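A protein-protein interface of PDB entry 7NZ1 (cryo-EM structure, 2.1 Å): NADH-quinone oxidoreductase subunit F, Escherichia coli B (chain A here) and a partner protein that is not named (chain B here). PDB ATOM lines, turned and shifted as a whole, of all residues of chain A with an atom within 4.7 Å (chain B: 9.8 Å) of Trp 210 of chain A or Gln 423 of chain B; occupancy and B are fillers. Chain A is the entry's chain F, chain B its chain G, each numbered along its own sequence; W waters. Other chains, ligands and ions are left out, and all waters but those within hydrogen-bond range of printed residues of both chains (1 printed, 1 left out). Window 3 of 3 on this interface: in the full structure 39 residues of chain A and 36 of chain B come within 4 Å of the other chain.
Trp 210 of chain A touches just one residue of chain B: Gln 423 (3.4 Å).
Gln 423 of chain B touches just these residues of chain A: Glu 191 (3.7 Å), Trp 210 (3.4 Å) and Gly 211 (3.97 Å).
Printed residues of chain B within 4 Å of Gly 208 of chain A: Asn 420.
Ala 209 of chain A touches none of the printed residues of chain B.
Of chain B, only Asn 420 (3.3 Å) and Gln 423 (3.97 Å) come within 4 Å of Gly 211 of chain A.
No residue of chain B comes within 4 Å of Lys 212 of chain A.
Printed residues of chain A within 4 Å of Asn 420 of chain B: Glu 191, Gly 208 and Gly 211.
The side-chain carboxylate of Glu 191 of chain A is in hydrogen-bond range of the backbone NH of Trp 210 of chain A.
The backbone carbonyl oxygen of Trp 210 of chain A sits at hydrogen-bond distance from the side-chain amino group of Lys 212 of chain A, 3.1 Å away.
The backbone carbonyl oxygen (O) of Asn 420 of chain B is in hydrogen-bond range of the side-chain amide nitrogen (NE2) of Gln 423 of chain B (3.2 Å).
Among the printed residues, pairs that only touch across the chains: Glu 191 of chain A with Asn 420 of chain B (3.6 Å), Glu 191 of chain A with Gln 423 of chain B (3.7 Å), Trp 210 of chain A with Gln 423 of chain B (3.4 Å), Gly 211 of chain A with Asn 420 of chain B (3.3 Å) and Gly 211 of chain A with Gln 423 of chain B (3.97 Å).
Water W1 bridges the backbone carbonyl oxygen (O) of Ile 421 of chain B (2.6 Å) and the backbone carbonyl oxygen (O) of Gly 211 of chain A (2.6 Å).
Of the 9 printed residues of chain A, 4 touch a printed residue of chain B.
Hydrophobic or aromatic side chains of chain A that line the printed part of chain B: Trp 210.
Along chain A the printed residues that touch a printed residue of chain B span positions 191 to 211.
Along chain B the printed residues that touch a printed residue of chain A span positions 420 to 423.
Among the printed residues, 6 pairs touch across the chains.
The backbone carbonyl oxygen (O) of Gly 208 of chain A lies close to the side-chain amide oxygen (OD1) of Asn 420 of chain B, at 3.4 Å.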
ATOM      1  N   TYR A  86       8.908 -29.159  18.864  1.00  0.00           N
ATOM      2  CA  TYR A  86      10.293 -28.944  19.255  1.00  0.00           C
ATOM      3  C   TYR A  86      10.880 -30.170  19.938  1.00  0.00           C
ATOM      4  O   TYR A  86      10.187 -30.902  20.650  1.00  0.00           O
ATOM      5  CB  TYR A  86      10.426 -27.750  20.194  1.00  0.00           C
ATOM      6  CG  TYR A  86      10.052 -26.461  19.531  1.00  0.00           C
ATOM      7  CD1 TYR A  86      10.905 -25.866  18.614  1.00  0.00           C
ATOM      8  CD2 TYR A  86       8.844 -25.837  19.819  1.00  0.00           C
ATOM      9  CE1 TYR A  86      10.571 -24.691  18.000  1.00  0.00           C
ATOM     10  CE2 TYR A  86       8.498 -24.657  19.210  1.00  0.00           C
ATOM     11  CZ  TYR A  86       9.369 -24.092  18.301  1.00  0.00           C
ATOM     12  OH  TYR A  86       9.040 -22.926  17.680  1.00  0.00           O
ATOM     13  N   TYR A 129      16.986 -27.704  19.873  1.00  0.00           N
ATOM     14  CA  TYR A 129      17.842 -26.879  20.715  1.00  0.00           C
ATOM     15  C   TYR A 129      18.626 -27.755  21.681  1.00  0.00           C
ATOM     16  O   TYR A 129      18.042 -28.572  22.398  1.00  0.00           O
ATOM     17  CB  TYR A 129      17.022 -25.850  21.498  1.00  0.00           C
ATOM     18  CG  TYR A 129      16.248 -24.884  20.636  1.00  0.00           C
ATOM     19  CD1 TYR A 129      16.842 -23.725  20.156  1.00  0.00           C
ATOM     20  CD2 TYR A 129      14.918 -25.125  20.311  1.00  0.00           C
ATOM     21  CE1 TYR A 129      16.136 -22.832  19.370  1.00  0.00           C
ATOM     22  CE2 TYR A 129      14.204 -24.241  19.524  1.00  0.00           C
ATOM     23  CZ  TYR A 129      14.822 -23.099  19.053  1.00  0.00           C
ATOM     24  OH  TYR A 129      14.123 -22.214  18.276  1.00  0.00           O
ATOM     25  N   LEU A 190      14.670 -21.741  28.376  1.00  0.00           N
ATOM     26  CA  LEU A 190      14.784 -21.607  26.925  1.00  0.00           C
ATOM     27  C   LEU A 190      13.952 -20.445  26.401  1.00  0.00           C
ATOM     28  O   LEU A 190      14.375 -19.730  25.488  1.00  0.00           O
ATOM     29  CB  LEU A 190      14.352 -22.903  26.247  1.00  0.00           C
ATOM     30  CG  LEU A 190      14.634 -22.978  24.748  1.00  0.00           C
ATOM     31  CD1 LEU A 190      16.095 -23.297  24.493  1.00  0.00           C
ATOM     32  CD2 LEU A 190      13.718 -23.967  24.065  1.00  0.00           C
ATOM     33  N   GLU A 191      12.777 -20.225  26.992  1.00  0.00           N
ATOM     34  CA  GLU A 191      11.894 -19.119  26.640  1.00  0.00           C
ATOM     35  C   GLU A 191      12.419 -17.758  27.082  1.00  0.00           C
ATOM     36  O   GLU A 191      11.809 -16.742  26.740  1.00  0.00           O
ATOM     37  CB  GLU A 191      10.516 -19.359  27.245  1.00  0.00           C
ATOM     38  CG  GLU A 191       9.687 -20.369  26.478  1.00  0.00           C
ATOM     39  CD  GLU A 191       8.272 -20.455  26.990  1.00  0.00           C
ATOM     40  OE1 GLU A 191       7.974 -19.803  28.011  1.00  0.00           O
ATOM     41  OE2 GLU A 191       7.479 -21.217  26.412  1.00  0.00           O
ATOM     42  N   GLY A 208       4.379 -27.296  25.617  1.00  0.00           N
ATOM     43  CA  GLY A 208       5.752 -27.100  26.040  1.00  0.00           C
ATOM     44  C   GLY A 208       6.309 -25.733  25.698  1.00  0.00           C
ATOM     45  O   GLY A 208       5.787 -24.713  26.155  1.00  0.00           O
ATOM     46  N   ALA A 209       7.398 -25.713  24.928  1.00  0.00           N
ATOM     47  CA  ALA A 209       8.076 -24.471  24.566  1.00  0.00           C
ATOM     48  C   ALA A 209       7.203 -23.626  23.647  1.00  0.00           C
ATOM     49  O   ALA A 209       6.818 -24.081  22.566  1.00  0.00           O
ATOM     50  CB  ALA A 209       9.413 -24.779  23.902  1.00  0.00           C
ATOM     51  N   TRP A 210       6.914 -22.396  24.093  1.00  0.00           N
ATOM     52  CA  TRP A 210       6.048 -21.426  23.410  1.00  0.00           C
ATOM     53  C   TRP A 210       4.667 -22.008  23.107  1.00  0.00           C
ATOM     54  O   TRP A 210       4.073 -21.736  22.064  1.00  0.00           O
ATOM     55  CB  TRP A 210       6.720 -20.866  22.152  1.00  0.00           C
ATOM     56  CG  TRP A 210       8.060 -20.269  22.446  1.00  0.00           C
ATOM     57  CD1 TRP A 210       8.306 -19.081  23.064  1.00  0.00           C
ATOM     58  CD2 TRP A 210       9.339 -20.830  22.135  1.00  0.00           C
ATOM     59  NE1 TRP A 210       9.657 -18.866  23.161  1.00  0.00           N
ATOM     60  CE2 TRP A 210      10.314 -19.925  22.596  1.00  0.00           C
ATOM     61  CE3 TRP A 210       9.754 -22.008  21.510  1.00  0.00           C
ATOM     62  CZ2 TRP A 210      11.679 -20.164  22.456  1.00  0.00           C
ATOM     63  CZ3 TRP A 210      11.107 -22.243  21.372  1.00  0.00           C
ATOM     64  CH2 TRP A 210      12.052 -21.327  21.843  1.00  0.00           C
ATOM     65  N   GLY A 211       4.159 -22.806  24.049  1.00  0.00           N
ATOM     66  CA  GLY A 211       2.879 -23.482  23.920  1.00  0.00           C
ATOM     67  C   GLY A 211       2.788 -24.430  22.749  1.00  0.00           C
ATOM     68  O   GLY A 211       1.714 -24.583  22.167  1.00  0.00           O
ATOM     69  N   LYS A 212       3.884 -25.083  22.400  1.00  0.00           N
ATOM     70  CA  LYS A 212       3.956 -26.012  21.289  1.00  0.00           C
ATOM     71  C   LYS A 212       4.301 -27.384  21.845  1.00  0.00           C
ATOM     72  O   LYS A 212       4.808 -27.485  22.966  1.00  0.00           O
ATOM     73  CB  LYS A 212       5.014 -25.564  20.269  1.00  0.00           C
ATOM     74  CG  LYS A 212       4.774 -24.177  19.719  1.00  0.00           C
ATOM     75  CD  LYS A 212       3.458 -24.091  18.985  1.00  0.00           C
ATOM     76  CE  LYS A 212       3.370 -22.807  18.188  1.00  0.00           C
ATOM     77  NZ  LYS A 212       3.506 -21.611  19.062  1.00  0.00           N
ATOM     78  N   LYS B 398      -7.722 -11.120  26.952  1.00  0.00           N
ATOM     79  CA  LYS B 398      -7.103 -12.385  27.325  1.00  0.00           C
ATOM     80  C   LYS B 398      -8.020 -13.577  27.096  1.00  0.00           C
ATOM     81  O   LYS B 398      -7.608 -14.713  27.347  1.00  0.00           O
ATOM     82  CB  LYS B 398      -6.675 -12.344  28.792  1.00  0.00           C
ATOM     83  CG  LYS B 398      -5.521 -11.422  29.047  1.00  0.00           C
ATOM     84  CD  LYS B 398      -5.277 -11.232  30.516  1.00  0.00           C
ATOM     85  CE  LYS B 398      -4.531  -9.944  30.735  1.00  0.00           C
ATOM     86  NZ  LYS B 398      -4.545  -9.535  32.150  1.00  0.00           N
ATOM     87  N   LYS B 400      -8.888 -14.891  24.338  1.00  0.00           N
ATOM     88  CA  LYS B 400      -8.405 -15.746  23.259  1.00  0.00           C
ATOM     89  C   LYS B 400      -7.587 -16.914  23.801  1.00  0.00           C
ATOM     90  O   LYS B 400      -7.741 -18.052  23.342  1.00  0.00           O
ATOM     91  CB  LYS B 400      -7.588 -14.910  22.272  1.00  0.00           C
ATOM     92  CG  LYS B 400      -6.773 -15.689  21.262  1.00  0.00           C
ATOM     93  CD  LYS B 400      -7.667 -16.406  20.270  1.00  0.00           C
ATOM     94  CE  LYS B 400      -6.989 -16.554  18.923  1.00  0.00           C
ATOM     95  NZ  LYS B 400      -6.188 -15.342  18.574  1.00  0.00           N
ATOM     96  N   ALA B 401      -6.738 -16.651  24.798  1.00  0.00           N
ATOM     97  CA  ALA B 401      -5.963 -17.710  25.433  1.00  0.00           C
ATOM     98  C   ALA B 401      -6.848 -18.669  26.219  1.00  0.00           C
ATOM     99  O   ALA B 401      -6.543 -19.864  26.287  1.00  0.00           O
ATOM    100  CB  ALA B 401      -4.897 -17.107  26.348  1.00  0.00           C
ATOM    101  N   ARG B 402      -7.940 -18.169  26.808  1.00  0.00           N
ATOM    102  CA  ARG B 402      -8.882 -19.046  27.498  1.00  0.00           C
ATOM    103  C   ARG B 402      -9.625 -19.963  26.530  1.00  0.00           C
ATOM    104  O   ARG B 402      -9.966 -21.091  26.900  1.00  0.00           O
ATOM    105  CB  ARG B 402      -9.874 -18.219  28.318  1.00  0.00           C
ATOM    106  CG  ARG B 402      -9.226 -17.342  29.383  1.00  0.00           C
ATOM    107  CD  ARG B 402     -10.246 -16.722  30.324  1.00  0.00           C
ATOM    108  NE  ARG B 402     -11.064 -15.682  29.706  1.00  0.00           N
ATOM    109  CZ  ARG B 402     -10.840 -14.380  29.819  1.00  0.00           C
ATOM    110  NH1 ARG B 402      -9.822 -13.911  30.517  1.00  0.00           N
ATOM    111  NH2 ARG B 402     -11.677 -13.524  29.239  1.00  0.00           N
ATOM    112  N   MET B 404      -8.391 -21.162  23.555  1.00  0.00           N
ATOM    113  CA  MET B 404      -7.430 -22.169  23.104  1.00  0.00           C
ATOM    114  C   MET B 404      -7.201 -23.239  24.164  1.00  0.00           C
ATOM    115  O   MET B 404      -7.120 -24.432  23.845  1.00  0.00           O
ATOM    116  CB  MET B 404      -6.108 -21.498  22.736  1.00  0.00           C
ATOM    117  CG  MET B 404      -6.141 -20.693  21.448  1.00  0.00           C
ATOM    118  SD  MET B 404      -4.819 -19.466  21.364  1.00  0.00           S
ATOM    119  CE  MET B 404      -3.370 -20.516  21.304  1.00  0.00           C
ATOM    120  N   ALA B 405      -7.082 -22.825  25.430  1.00  0.00           N
ATOM    121  CA  ALA B 405      -6.860 -23.761  26.529  1.00  0.00           C
ATOM    122  C   ALA B 405      -8.066 -24.667  26.762  1.00  0.00           C
ATOM    123  O   ALA B 405      -7.902 -25.838  27.119  1.00  0.00           O
ATOM    124  CB  ALA B 405      -6.513 -22.995  27.803  1.00  0.00           C
ATOM    125  N   GLN B 408      -8.034 -27.568  24.526  1.00  0.00           N
ATOM    126  CA  GLN B 408      -7.034 -28.544  24.933  1.00  0.00           C
ATOM    127  C   GLN B 408      -7.330 -29.167  26.294  1.00  0.00           C
ATOM    128  O   GLN B 408      -6.457 -29.845  26.845  1.00  0.00           O
ATOM    129  CB  GLN B 408      -5.649 -27.897  24.931  1.00  0.00           C
ATOM    130  CG  GLN B 408      -5.127 -27.624  23.536  1.00  0.00           C
ATOM    131  CD  GLN B 408      -3.643 -27.344  23.502  1.00  0.00           C
ATOM    132  OE1 GLN B 408      -2.838 -28.145  23.970  1.00  0.00           O
ATOM    133  NE2 GLN B 408      -3.270 -26.210  22.927  1.00  0.00           N
ATOM    134  N   ILE B 415      -3.868 -21.140  35.791  1.00  0.00           N
ATOM    135  CA  ILE B 415      -3.619 -19.911  35.043  1.00  0.00           C
ATOM    136  C   ILE B 415      -2.277 -19.956  34.305  1.00  0.00           C
ATOM    137  O   ILE B 415      -2.174 -19.450  33.182  1.00  0.00           O
ATOM    138  CB  ILE B 415      -3.746 -18.693  35.988  1.00  0.00           C
ATOM    139  CG1 ILE B 415      -3.502 -17.363  35.259  1.00  0.00           C
ATOM    140  CG2 ILE B 415      -2.873 -18.831  37.224  1.00  0.00           C
ATOM    141  CD1 ILE B 415      -4.431 -17.112  34.107  1.00  0.00           C
ATOM    142  N   ALA B 416      -1.254 -20.596  34.880  1.00  0.00           N
ATOM    143  CA  ALA B 416       0.049 -20.650  34.225  1.00  0.00           C
ATOM    144  C   ALA B 416       0.033 -21.551  32.994  1.00  0.00           C
ATOM    145  O   ALA B 416       0.805 -21.327  32.058  1.00  0.00           O
ATOM    146  CB  ALA B 416       1.113 -21.118  35.211  1.00  0.00           C
ATOM    147  N   ALA B 417      -0.848 -22.552  32.967  1.00  0.00           N
ATOM    148  CA  ALA B 417      -1.004 -23.370  31.769  1.00  0.00           C
ATOM    149  C   ALA B 417      -1.721 -22.604  30.663  1.00  0.00           C
ATOM    150  O   ALA B 417      -1.359 -22.726  29.488  1.00  0.00           O
ATOM    151  CB  ALA B 417      -1.746 -24.662  32.107  1.00  0.00           C
ATOM    152  N   ILE B 418      -2.747 -21.825  31.027  1.00  0.00           N
ATOM    153  CA  ILE B 418      -3.498 -21.021  30.062  1.00  0.00           C
ATOM    154  C   ILE B 418      -2.605 -19.949  29.443  1.00  0.00           C
ATOM    155  O   ILE B 418      -2.634 -19.721  28.227  1.00  0.00           O
ATOM    156  CB  ILE B 418      -4.738 -20.408  30.744  1.00  0.00           C
ATOM    157  CG1 ILE B 418      -5.720 -21.502  31.158  1.00  0.00           C
ATOM    158  CG2 ILE B 418      -5.430 -19.381  29.857  1.00  0.00           C
ATOM    159  CD1 ILE B 418      -6.713 -21.056  32.186  1.00  0.00           C
ATOM    160  N   LEU B 419      -1.783 -19.295  30.269  1.00  0.00           N
ATOM    161  CA  LEU B 419      -0.871 -18.269  29.774  1.00  0.00           C
ATOM    162  C   LEU B 419       0.217 -18.851  28.878  1.00  0.00           C
ATOM    163  O   LEU B 419       0.637 -18.195  27.919  1.00  0.00           O
ATOM    164  CB  LEU B 419      -0.239 -17.516  30.945  1.00  0.00           C
ATOM    165  CG  LEU B 419      -1.146 -16.583  31.757  1.00  0.00           C
ATOM    166  CD1 LEU B 419      -0.339 -15.821  32.792  1.00  0.00           C
ATOM    167  CD2 LEU B 419      -1.914 -15.633  30.860  1.00  0.00           C
ATOM    168  N   ASN B 420       0.666 -20.079  29.160  1.00  0.00           N
ATOM    169  CA  ASN B 420       1.654 -20.727  28.298  1.00  0.00           C
ATOM    170  C   ASN B 420       1.063 -21.107  26.942  1.00  0.00           C
ATOM    171  O   ASN B 420       1.760 -21.051  25.925  1.00  0.00           O
ATOM    172  CB  ASN B 420       2.241 -21.957  28.987  1.00  0.00           C
ATOM    173  CG  ASN B 420       3.181 -22.729  28.085  1.00  0.00           C
ATOM    174  OD1 ASN B 420       2.882 -23.843  27.665  1.00  0.00           O
ATOM    175  ND2 ASN B 420       4.302 -22.112  27.739  1.00  0.00           N
ATOM    176  N   ILE B 421      -0.203 -21.534  26.913  1.00  0.00           N
ATOM    177  CA  ILE B 421      -0.855 -21.884  25.651  1.00  0.00           C
ATOM    178  C   ILE B 421      -1.066 -20.643  24.784  1.00  0.00           C
ATOM    179  O   ILE B 421      -0.868 -20.684  23.564  1.00  0.00           O
ATOM    180  CB  ILE B 421      -2.168 -22.647  25.934  1.00  0.00           C
ATOM    181  CG1 ILE B 421      -1.855 -24.056  26.427  1.00  0.00           C
ATOM    182  CG2 ILE B 421      -3.061 -22.766  24.708  1.00  0.00           C
ATOM    183  CD1 ILE B 421      -2.943 -24.655  27.259  1.00  0.00           C
ATOM    184  N   GLY B 422      -1.410 -19.511  25.406  1.00  0.00           N
ATOM    185  CA  GLY B 422      -1.695 -18.264  24.714  1.00  0.00           C
ATOM    186  C   GLY B 422      -0.590 -17.678  23.851  1.00  0.00           C
ATOM    187  O   GLY B 422      -0.769 -17.591  22.632  1.00  0.00           O
ATOM    188  N   GLN B 423       0.534 -17.294  24.471  1.00  0.00           N
ATOM    189  CA  GLN B 423       1.757 -16.801  23.816  1.00  0.00           C
ATOM    190  C   GLN B 423       1.474 -15.576  22.939  1.00  0.00           C
ATOM    191  O   GLN B 423       1.545 -15.628  21.708  1.00  0.00           O
ATOM    192  CB  GLN B 423       2.436 -17.892  22.979  1.00  0.00           C
ATOM    193  CG  GLN B 423       3.058 -19.001  23.764  1.00  0.00           C
ATOM    194  CD  GLN B 423       4.233 -18.565  24.601  1.00  0.00           C
ATOM    195  OE1 GLN B 423       4.982 -17.666  24.223  1.00  0.00           O
ATOM    196  NE2 GLN B 423       4.405 -19.207  25.745  1.00  0.00           N
ATOM    197  N   ARG B 424       1.084 -14.493  23.615  1.00  0.00           N
ATOM    198  CA  ARG B 424       0.805 -13.163  23.067  1.00  0.00           C
ATOM    199  C   ARG B 424      -0.383 -13.121  22.101  1.00  0.00           C
ATOM    200  O   ARG B 424      -0.611 -12.086  21.470  1.00  0.00           O
ATOM    201  CB  ARG B 424       2.039 -12.531  22.391  1.00  0.00           C
ATOM    202  CG  ARG B 424       3.320 -12.577  23.212  1.00  0.00           C
ATOM    203  CD  ARG B 424       4.445 -11.819  22.530  1.00  0.00           C
ATOM    204  NE  ARG B 424       5.069 -12.588  21.462  1.00  0.00           N
ATOM    205  CZ  ARG B 424       6.032 -12.130  20.674  1.00  0.00           C
ATOM    206  NH1 ARG B 424       6.509 -10.904  20.806  1.00  0.00           N
ATOM    207  NH2 ARG B 424       6.523 -12.920  19.725  1.00  0.00           N
ATOM    208  N   ALA B 425      -1.145 -14.204  21.959  1.00  0.00           N
ATOM    209  CA  ALA B 425      -2.373 -14.155  21.176  1.00  0.00           C
ATOM    210  C   ALA B 425      -3.438 -13.384  21.946  1.00  0.00           C
ATOM    211  O   ALA B 425      -3.636 -13.604  23.142  1.00  0.00           O
ATOM    212  CB  ALA B 425      -2.865 -15.563  20.854  1.00  0.00           C
ATOM    213  N   LYS B 426      -4.110 -12.466  21.260  1.00  0.00           N
ATOM    214  CA  LYS B 426      -5.039 -11.552  21.902  1.00  0.00           C
ATOM    215  C   LYS B 426      -6.315 -11.466  21.081  1.00  0.00           C
ATOM    216  O   LYS B 426      -6.296 -11.621  19.858  1.00  0.00           O
ATOM    217  CB  LYS B 426      -4.436 -10.147  22.060  1.00  0.00           C
ATOM    218  CG  LYS B 426      -3.224 -10.046  22.978  1.00  0.00           C
ATOM    219  CD  LYS B 426      -2.639  -8.647  22.982  1.00  0.00           C
ATOM    220  CE  LYS B 426      -1.532  -8.505  24.013  1.00  0.00           C
ATOM    221  NZ  LYS B 426      -1.903  -9.065  25.343  1.00  0.00           N
HETATM  222  O   HOH W   1      -0.083 -22.656  22.069  1.00  0.00           O
